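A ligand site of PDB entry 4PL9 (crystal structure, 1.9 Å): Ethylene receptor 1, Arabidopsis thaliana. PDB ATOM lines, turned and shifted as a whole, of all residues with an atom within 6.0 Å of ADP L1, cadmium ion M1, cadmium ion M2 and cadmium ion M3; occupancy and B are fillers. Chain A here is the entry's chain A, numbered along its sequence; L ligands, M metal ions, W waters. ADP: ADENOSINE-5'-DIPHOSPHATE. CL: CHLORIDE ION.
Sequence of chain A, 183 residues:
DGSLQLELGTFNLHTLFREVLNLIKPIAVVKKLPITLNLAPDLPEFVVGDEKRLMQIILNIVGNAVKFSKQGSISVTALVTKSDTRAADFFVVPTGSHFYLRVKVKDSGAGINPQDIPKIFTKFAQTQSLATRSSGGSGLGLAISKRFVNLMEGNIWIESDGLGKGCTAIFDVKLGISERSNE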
ATOM      1  N   ASN A  60      24.548  20.450   3.053  1.00  0.00           N
ATOM      2  CA  ASN A  60      23.556  21.505   3.107  1.00  0.00           C
ATOM      3  C   ASN A  60      22.401  21.292   2.166  1.00  0.00           C
ATOM      4  O   ASN A  60      21.277  21.624   2.523  1.00  0.00           O
ATOM      5  CB  ASN A  60      24.124  22.901   2.939  1.00  0.00           C
ATOM      6  CG  ASN A  60      23.023  23.966   2.915  1.00  0.00           C
ATOM      7  OD1 ASN A  60      22.295  24.192   3.910  1.00  0.00           O
ATOM      8  ND2 ASN A  60      22.869  24.591   1.761  1.00  0.00           N
ATOM      9  N   ILE A  61      22.615  20.721   0.981  1.00  0.00           N
ATOM     10  CA  ILE A  61      21.502  20.512   0.071  1.00  0.00           C
ATOM     11  C   ILE A  61      20.605  19.350   0.494  1.00  0.00           C
ATOM     12  O   ILE A  61      19.375  19.458   0.409  1.00  0.00           O
ATOM     13  CB  ILE A  61      21.944  20.386  -1.411  1.00  0.00           C
ATOM     14  CG1 ILE A  61      22.293  21.776  -1.940  1.00  0.00           C
ATOM     15  CG2 ILE A  61      20.846  19.827  -2.230  1.00  0.00           C
ATOM     16  CD1 ILE A  61      23.361  21.762  -2.987  1.00  0.00           C
ATOM     17  N   GLY A  63      20.399  18.353   3.554  1.00  0.00           N
ATOM     18  CA  GLY A  63      19.845  18.862   4.800  1.00  0.00           C
ATOM     19  C   GLY A  63      18.660  19.804   4.577  1.00  0.00           C
ATOM     20  O   GLY A  63      17.660  19.779   5.312  1.00  0.00           O
ATOM     21  N   ASN A  64      18.775  20.664   3.566  1.00  0.00           N
ATOM     22  CA  ASN A  64      17.656  21.517   3.183  1.00  0.00           C
ATOM     23  C   ASN A  64      16.411  20.758   2.810  1.00  0.00           C
ATOM     24  O   ASN A  64      15.292  21.177   3.139  1.00  0.00           O
ATOM     25  CB  ASN A  64      18.047  22.440   2.060  1.00  0.00           C
ATOM     26  CG  ASN A  64      18.840  23.634   2.539  1.00  0.00           C
ATOM     27  OD1 ASN A  64      18.764  23.990   3.715  1.00  0.00           O
ATOM     28  ND2 ASN A  64      19.565  24.279   1.635  1.00  0.00           N
ATOM     29  N   ALA A  65      16.581  19.657   2.083  1.00  0.00           N
ATOM     30  CA  ALA A  65      15.455  18.831   1.669  1.00  0.00           C
ATOM     31  C   ALA A  65      14.700  18.319   2.889  1.00  0.00           C
ATOM     32  O   ALA A  65      13.471  18.347   2.926  1.00  0.00           O
ATOM     33  CB  ALA A  65      15.920  17.663   0.794  1.00  0.00           C
ATOM     34  N   LYS A  67      14.930  19.649   6.004  1.00  0.00           N
ATOM     35  CA  LYS A  67      14.471  20.828   6.737  1.00  0.00           C
ATOM     36  C   LYS A  67      13.166  21.415   6.192  1.00  0.00           C
ATOM     37  O   LYS A  67      12.271  21.758   6.963  1.00  0.00           O
ATOM     38  CB  LYS A  67      15.575  21.875   6.714  1.00  0.00           C
ATOM     39  CG  LYS A  67      15.303  23.165   7.474  1.00  0.00           C
ATOM     40  CD  LYS A  67      16.461  24.138   7.171  1.00  0.00           C
ATOM     41  CE  LYS A  67      16.319  25.470   7.898  1.00  0.00           C
ATOM     42  NZ  LYS A  67      17.404  26.436   7.512  1.00  0.00           N
ATOM     43  N   PHE A  68      13.068  21.539   4.859  1.00  0.00           N
ATOM     44  CA  PHE A  68      11.953  22.250   4.251  1.00  0.00           C
ATOM     45  C   PHE A  68      10.824  21.340   3.804  1.00  0.00           C
ATOM     46  O   PHE A  68       9.821  21.806   3.263  1.00  0.00           O
ATOM     47  CB  PHE A  68      12.467  23.091   3.093  1.00  0.00           C
ATOM     48  CG  PHE A  68      13.294  24.250   3.541  1.00  0.00           C
ATOM     49  CD1 PHE A  68      12.706  25.296   4.250  1.00  0.00           C
ATOM     50  CD2 PHE A  68      14.654  24.274   3.298  1.00  0.00           C
ATOM     51  CE1 PHE A  68      13.477  26.370   4.695  1.00  0.00           C
ATOM     52  CE2 PHE A  68      15.433  25.348   3.723  1.00  0.00           C
ATOM     53  CZ  PHE A  68      14.836  26.398   4.433  1.00  0.00           C
ATOM     54  N   SER A  69      10.966  20.050   4.031  1.00  0.00           N
ATOM     55  CA  SER A  69       9.884  19.124   3.724  1.00  0.00           C
ATOM     56  C   SER A  69       9.117  18.773   4.987  1.00  0.00           C
ATOM     57  O   SER A  69       9.712  18.550   6.047  1.00  0.00           O
ATOM     58  CB  SER A  69      10.428  17.868   3.062  1.00  0.00           C
ATOM     59  OG  SER A  69      11.057  18.180   1.841  1.00  0.00           O
ATOM     60  N   ASP A 107      13.024  16.988  -3.231  1.00  0.00           N
ATOM     61  CA  ASP A 107      12.216  16.861  -2.019  1.00  0.00           C
ATOM     62  C   ASP A 107      10.735  16.987  -2.313  1.00  0.00           C
ATOM     63  O   ASP A 107      10.328  17.115  -3.454  1.00  0.00           O
ATOM     64  CB  ASP A 107      12.672  17.830  -0.913  1.00  0.00           C
ATOM     65  CG  ASP A 107      12.358  19.291  -1.204  1.00  0.00           C
ATOM     66  OD1 ASP A 107      11.392  19.623  -1.938  1.00  0.00           O
ATOM     67  OD2 ASP A 107      13.082  20.120  -0.617  1.00  0.00           O
ATOM     68  N   SER A 108       9.939  16.930  -1.259  1.00  0.00           N
ATOM     69  CA  SER A 108       8.496  16.942  -1.378  1.00  0.00           C
ATOM     70  C   SER A 108       7.907  18.130  -0.631  1.00  0.00           C
ATOM     71  O   SER A 108       6.835  18.010  -0.045  1.00  0.00           O
ATOM     72  CB  SER A 108       7.962  15.641  -0.791  1.00  0.00           C
ATOM     73  OG  SER A 108       8.627  15.369   0.441  1.00  0.00           O
ATOM     74  N   GLY A 109       8.612  19.250  -0.617  1.00  0.00           N
ATOM     75  CA  GLY A 109       8.120  20.454   0.040  1.00  0.00           C
ATOM     76  C   GLY A 109       6.930  21.095  -0.679  1.00  0.00           C
ATOM     77  O   GLY A 109       6.344  20.552  -1.615  1.00  0.00           O
ATOM     78  N   ALA A 110       6.586  22.291  -0.213  1.00  0.00           N
ATOM     79  CA  ALA A 110       5.416  23.010  -0.693  1.00  0.00           C
ATOM     80  C   ALA A 110       5.681  23.709  -2.031  1.00  0.00           C
ATOM     81  O   ALA A 110       4.769  24.301  -2.622  1.00  0.00           O
ATOM     82  CB  ALA A 110       4.991  24.030   0.348  1.00  0.00           C
ATOM     83  N   GLY A 111       6.902  23.605  -2.524  1.00  0.00           N
ATOM     84  CA  GLY A 111       7.296  24.219  -3.773  1.00  0.00           C
ATOM     85  C   GLY A 111       7.904  25.588  -3.524  1.00  0.00           C
ATOM     86  O   GLY A 111       7.800  26.134  -2.430  1.00  0.00           O
ATOM     87  N   ILE A 112       8.566  26.124  -4.549  1.00  0.00           N
ATOM     88  CA  ILE A 112       9.169  27.449  -4.478  1.00  0.00           C
ATOM     89  C   ILE A 112       8.629  28.332  -5.618  1.00  0.00           C
ATOM     90  O   ILE A 112       8.668  27.925  -6.787  1.00  0.00           O
ATOM     91  CB  ILE A 112      10.713  27.372  -4.596  1.00  0.00           C
ATOM     92  CG1 ILE A 112      11.305  26.451  -3.509  1.00  0.00           C
ATOM     93  CG2 ILE A 112      11.327  28.750  -4.480  1.00  0.00           C
ATOM     94  CD1 ILE A 112      12.793  26.173  -3.681  1.00  0.00           C
ATOM     95  N   ILE A 120      17.669  33.162  -4.406  1.00  0.00           N
ATOM     96  CA  ILE A 120      17.844  32.101  -3.422  1.00  0.00           C
ATOM     97  C   ILE A 120      19.276  31.987  -2.896  1.00  0.00           C
ATOM     98  O   ILE A 120      19.476  31.469  -1.796  1.00  0.00           O
ATOM     99  CB  ILE A 120      17.377  30.741  -3.961  1.00  0.00           C
ATOM    100  CG1 ILE A 120      16.332  30.147  -3.018  1.00  0.00           C
ATOM    101  CG2 ILE A 120      18.549  29.800  -4.112  1.00  0.00           C
ATOM    102  CD1 ILE A 120      15.751  28.860  -3.504  1.00  0.00           C
ATOM    103  N   LYS A 123      19.664  35.456  -0.299  1.00  0.00           N
ATOM    104  CA  LYS A 123      18.450  35.755   0.465  1.00  0.00           C
ATOM    105  C   LYS A 123      18.691  36.503   1.795  1.00  0.00           C
ATOM    106  O   LYS A 123      17.732  36.877   2.492  1.00  0.00           O
ATOM    107  CB  LYS A 123      17.676  34.464   0.716  1.00  0.00           C
ATOM    108  CG  LYS A 123      16.170  34.632   0.631  1.00  0.00           C
ATOM    109  CD  LYS A 123      15.430  33.469   1.259  1.00  0.00           C
ATOM    110  CE  LYS A 123      13.957  33.794   1.443  1.00  0.00           C
ATOM    111  NZ  LYS A 123      13.232  32.746   2.227  1.00  0.00           N
ATOM    112  N   SER A 138      17.706  35.355   5.965  1.00  0.00           N
ATOM    113  CA  SER A 138      18.472  34.549   6.915  1.00  0.00           C
ATOM    114  C   SER A 138      18.863  33.206   6.284  1.00  0.00           C
ATOM    115  O   SER A 138      18.014  32.489   5.760  1.00  0.00           O
ATOM    116  CB  SER A 138      17.636  34.306   8.179  1.00  0.00           C
ATOM    117  OG  SER A 138      16.706  33.237   8.006  1.00  0.00           O
ATOM    118  N   GLY A 139      20.144  32.879   6.330  1.00  0.00           N
ATOM    119  CA  GLY A 139      20.612  31.547   5.940  1.00  0.00           C
ATOM    120  C   GLY A 139      21.822  31.575   5.016  1.00  0.00           C
ATOM    121  O   GLY A 139      21.828  32.320   4.047  1.00  0.00           O
ATOM    122  N   LEU A 140      22.841  30.760   5.285  1.00  0.00           N
ATOM    123  CA  LEU A 140      24.151  30.917   4.644  1.00  0.00           C
ATOM    124  C   LEU A 140      24.593  29.720   3.793  1.00  0.00           C
ATOM    125  O   LEU A 140      25.581  29.810   3.055  1.00  0.00           O
ATOM    126  CB  LEU A 140      25.242  31.194   5.697  1.00  0.00           C
ATOM    127  CG  LEU A 140      25.292  32.560   6.379  1.00  0.00           C
ATOM    128  CD1 LEU A 140      24.157  32.795   7.353  1.00  0.00           C
ATOM    129  CD2 LEU A 140      26.619  32.738   7.091  1.00  0.00           C
ATOM    130  N   GLY A 141      23.865  28.601   3.915  1.00  0.00           N
ATOM    131  CA  GLY A 141      24.272  27.343   3.327  1.00  0.00           C
ATOM    132  C   GLY A 141      24.503  27.385   1.832  1.00  0.00           C
ATOM    133  O   GLY A 141      25.535  26.893   1.340  1.00  0.00           O
ATOM    134  N   LEU A 142      23.556  27.958   1.080  1.00  0.00           N
ATOM    135  CA  LEU A 142      23.643  27.927  -0.370  1.00  0.00           C
ATOM    136  C   LEU A 142      24.660  28.945  -0.855  1.00  0.00           C
ATOM    137  O   LEU A 142      25.320  28.700  -1.855  1.00  0.00           O
ATOM    138  CB  LEU A 142      22.283  28.171  -1.008  1.00  0.00           C
ATOM    139  CG  LEU A 142      21.328  26.988  -0.962  1.00  0.00           C
ATOM    140  CD1 LEU A 142      20.009  27.362  -1.554  1.00  0.00           C
ATOM    141  CD2 LEU A 142      21.913  25.803  -1.667  1.00  0.00           C
ATOM    142  N   ALA A 143      24.785  30.082  -0.175  1.00  0.00           N
ATOM    143  CA  ALA A 143      25.799  31.058  -0.537  1.00  0.00           C
ATOM    144  C   ALA A 143      27.204  30.451  -0.445  1.00  0.00           C
ATOM    145  O   ALA A 143      28.066  30.652  -1.336  1.00  0.00           O
ATOM    146  CB  ALA A 143      25.689  32.275   0.335  1.00  0.00           C
ATOM    147  N   ILE A 158      18.640  25.679  -8.324  1.00  0.00           N
ATOM    148  CA  ILE A 158      17.451  25.080  -7.774  1.00  0.00           C
ATOM    149  C   ILE A 158      16.300  25.356  -8.706  1.00  0.00           C
ATOM    150  O   ILE A 158      16.232  26.407  -9.342  1.00  0.00           O
ATOM    151  CB  ILE A 158      17.158  25.646  -6.360  1.00  0.00           C
ATOM    152  CG1 ILE A 158      18.316  25.296  -5.427  1.00  0.00           C
ATOM    153  CG2 ILE A 158      15.827  25.141  -5.865  1.00  0.00           C
ATOM    154  CD1 ILE A 158      18.068  25.666  -3.944  1.00  0.00           C
ATOM    155  N   GLY A 166       7.343  20.422  -4.393  1.00  0.00           N
ATOM    156  CA  GLY A 166       8.710  20.404  -3.870  1.00  0.00           C
ATOM    157  C   GLY A 166       9.669  21.114  -4.801  1.00  0.00           C
ATOM    158  O   GLY A 166       9.265  21.979  -5.585  1.00  0.00           O
ATOM    159  N   CYS A 167      10.946  20.766  -4.709  1.00  0.00           N
ATOM    160  CA  CYS A 167      11.953  21.349  -5.571  1.00  0.00           C
ATOM    161  C   CYS A 167      13.049  20.330  -5.804  1.00  0.00           C
ATOM    162  O   CYS A 167      13.101  19.299  -5.122  1.00  0.00           O
ATOM    163  CB  CYS A 167      12.563  22.604  -4.939  1.00  0.00           C
ATOM    164  SG  CYS A 167      13.647  22.279  -3.542  1.00  0.00           S
ATOM    165  N   THR A 168      13.916  20.606  -6.769  1.00  0.00           N
ATOM    166  CA  THR A 168      15.122  19.831  -6.957  1.00  0.00           C
ATOM    167  C   THR A 168      16.315  20.772  -6.938  1.00  0.00           C
ATOM    168  O   THR A 168      16.322  21.822  -7.596  1.00  0.00           O
ATOM    169  CB  THR A 168      15.091  19.044  -8.270  1.00  0.00           C
ATOM    170  OG1 THR A 168      13.911  18.239  -8.294  1.00  0.00           O
ATOM    171  CG2 THR A 168      16.283  18.150  -8.377  1.00  0.00           C
ATOM    172  N   ALA A 169      17.305  20.442  -6.131  1.00  0.00           N
ATOM    173  CA  ALA A 169      18.554  21.165  -6.120  1.00  0.00           C
ATOM    174  C   ALA A 169      19.562  20.307  -6.867  1.00  0.00           C
ATOM    175  O   ALA A 169      19.681  19.117  -6.613  1.00  0.00           O
ATOM    176  CB  ALA A 169      19.014  21.449  -4.693  1.00  0.00           C
HETATM  177  PB  ADP L   1      18.788  28.423   5.159  1.00  0.00           P
HETATM  178  O1B ADP L   1      19.607  28.772   6.340  1.00  0.00           O
HETATM  179  O2B ADP L   1      18.408  26.985   5.002  1.00  0.00           O
HETATM  180  O3B ADP L   1      17.623  29.375   5.033  1.00  0.00           O
HETATM  181  PA  ADP L   1      20.128  28.197   2.558  1.00  0.00           P
HETATM  182  O1A ADP L   1      20.428  26.739   2.602  1.00  0.00           O
HETATM  183  O2A ADP L   1      21.142  29.088   1.893  1.00  0.00           O
HETATM  184  O3A ADP L   1      19.811  28.866   3.989  1.00  0.00           O
HETATM  185  O5' ADP L   1      18.719  28.353   1.825  1.00  0.00           O
HETATM  186  C5' ADP L   1      18.366  29.654   1.376  1.00  0.00           C
HETATM  187  C4' ADP L   1      16.867  29.667   1.196  1.00  0.00           C
HETATM  188  O4' ADP L   1      16.557  28.859   0.059  1.00  0.00           O
HETATM  189  C3' ADP L   1      16.108  29.012   2.346  1.00  0.00           C
HETATM  190  O3' ADP L   1      15.873  29.899   3.441  1.00  0.00           O
HETATM  191  C2' ADP L   1      14.828  28.594   1.641  1.00  0.00           C
HETATM  192  O2' ADP L   1      13.915  29.691   1.415  1.00  0.00           O
HETATM  193  C1' ADP L   1      15.324  28.184   0.278  1.00  0.00           C
HETATM  194  N9  ADP L   1      15.561  26.722   0.156  1.00  0.00           N
HETATM  195  C8  ADP L   1      16.762  26.113   0.106  1.00  0.00           C
HETATM  196  N7  ADP L   1      16.609  24.783  -0.047  1.00  0.00           N
HETATM  197  C5  ADP L   1      15.286  24.571  -0.104  1.00  0.00           C
HETATM  198  C6  ADP L   1      14.438  23.397  -0.275  1.00  0.00           C
HETATM  199  N6  ADP L   1      15.009  22.181  -0.387  1.00  0.00           N
HETATM  200  N1  ADP L   1      13.101  23.603  -0.281  1.00  0.00           N
HETATM  201  C2  ADP L   1      12.526  24.808  -0.161  1.00  0.00           C
HETATM  202  N3  ADP L   1      13.237  25.920  -0.004  1.00  0.00           N
HETATM  203  C4  ADP L   1      14.601  25.849   0.016  1.00  0.00           C
HETATM  204 CL    CL L   2       9.846  23.034  -1.721  1.00  0.00          CL
HETATM  205 CD    CD M   1      20.317  25.500   4.598  1.00  0.00          CD
HETATM  206 CD    CD M   2      20.820  27.563   7.920  1.00  0.00          CD
HETATM  207 CD    CD M   3      12.066  22.008  -1.714  1.00  0.00          CD
HETATM  208  O   HOH W   1      11.121  27.759   0.519  1.00  0.00           O
HETATM  209  O   HOH W   2      12.904  30.541   4.202  1.00  0.00           O
HETATM  210  O   HOH W   3      21.889  26.879   5.892  1.00  0.00           O
HETATM  211  O   HOH W   4      22.606  31.234   1.708  1.00  0.00           O
HETATM  212  O   HOH W   5      18.808  23.429  -1.207  1.00  0.00           O
HETATM  213  O   HOH W   6      17.696  20.875  -1.200  1.00  0.00           O
HETATM  214  O   HOH W   7      20.135  24.055   6.675  1.00  0.00           O
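Cadmium ion M3 is bound by N1 of ADP L1 (2.4 Å), OD2 of Asp 107 (2.4 Å), SG of Cys 167 (2.4 Å), CL of CL L2 (2.4 Å) and OD1 of Asp 107 (2.5 Å).
N of Gly 109 sits close to OD1 of Asp 107, 3.1 Å away. OG of Ser 69 is in hydrogen-bond range of O of Ala 65, at 2.7 Å.
The backbone carbonyl oxygen (O) of Ser 138 lies close to an oxygen (O3B) of ADP L1 (3.2 Å). Ala 65 touches ADP L1 (N to N6, 3.9 Å). Phe 68 touches ADP L1 (CB to N1, 3.5 Å). CD1 of Ile 112 touches N3 of ADP L1, at 3.7 Å. Ile 120 touches ADP L1 (CG1 to O4', 3.3 Å). Gly 139 touches ADP L1. N of Leu 140 touches O3A of ADP L1, at 3.8 Å. Hydrophobic or aromatic side chains that line ADP L1: Phe 68, Ile 112, Ile 120 and Leu 142. Within 4 Å of ADP L1: Asn 60, Asn 64, Ala 65, Lys 67, Phe 68, Asp 107, Ile 112, Ile 120, Lys 123, Ser 138, Gly 139, Leu 140, Gly 141, Leu 142 and Cys 167. The nearest printed residue that does not touch ADP L1 is Ile 158 (4.3 Å).
The backbone NH of Gly 141 sits at hydrogen-bond distance from an oxygen (O2A) of ADP L1. NZ of Lys 67 is in salt-bridge range of O3B of ADP L1 (3.9 Å). An oxygen (O2A) of ADP L1 sits at hydrogen-bond distance from the backbone NH (N) of Leu 142, 2.8 Å away. NZ of Lys 123 sits at hydrogen-bond distance from O2' of ADP L1.
Water W3 lies within hydrogen-bond range of N of Gly 141 (3.3 Å) and O3A of ADP L1 (3.4 Å). Water W4 lies within hydrogen-bond range of an oxygen (O2A) of ADP L1 (2.6 Å), the backbone carbonyl oxygen (O) of Gly 139 (2.7 Å), the backbone NH (N) of Ala 143 (3.1 Å) and the backbone NH (N) of Leu 142 (3.5 Å). Water W5 lies within hydrogen-bond range of N7 of ADP L1 and ND2 of Asn 64. Water W2 bridges the side-chain amino group (NZ) of Lys 123 (3.0 Å) and an oxygen (O2') of ADP L1 (3.1 Å). Water W6 lies within hydrogen-bond range of the backbone carbonyl oxygen (O) of Ile 61 (2.7 Å) and a nitrogen (N6) of ADP L1 (3.1 Å).
OD1 of Asn 64 binds cadmium ion M1 (2.3 Å). O1A of ADP L1 is bound to cadmium ion M1 (2.4 Å). O2B of ADP L1 binds cadmium ion M1 (2.5 Å). Water W3 is bound to cadmium ion M1, at 2.5 Å. Cadmium ion M1 is bound by OD1 of Asn 60. Cadmium ion M1 is bound by water W7 (2.5 Å). Cadmium ion M1 has six donor atoms within binding distance.
Merely in contact with cadmium ion M2: Lys 67 (3.6 Å). Of the 27 residues printed, 1 comes within 4 Å of cadmium ion M2.
O1B of ADP L1 binds cadmium ion M2, at 2.3 Å. Water W3 is bound to cadmium ion M2, at 2.4 Å.
Of the 27 residues printed, 2 come within 4 Å of cadmium ion M3. The nearest printed residue that does not touch cadmium ion M3 is Gly 166 (4.01 Å).
Along chain A the residues within 4 Å of cadmium ion M1 span positions 60 to 64.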
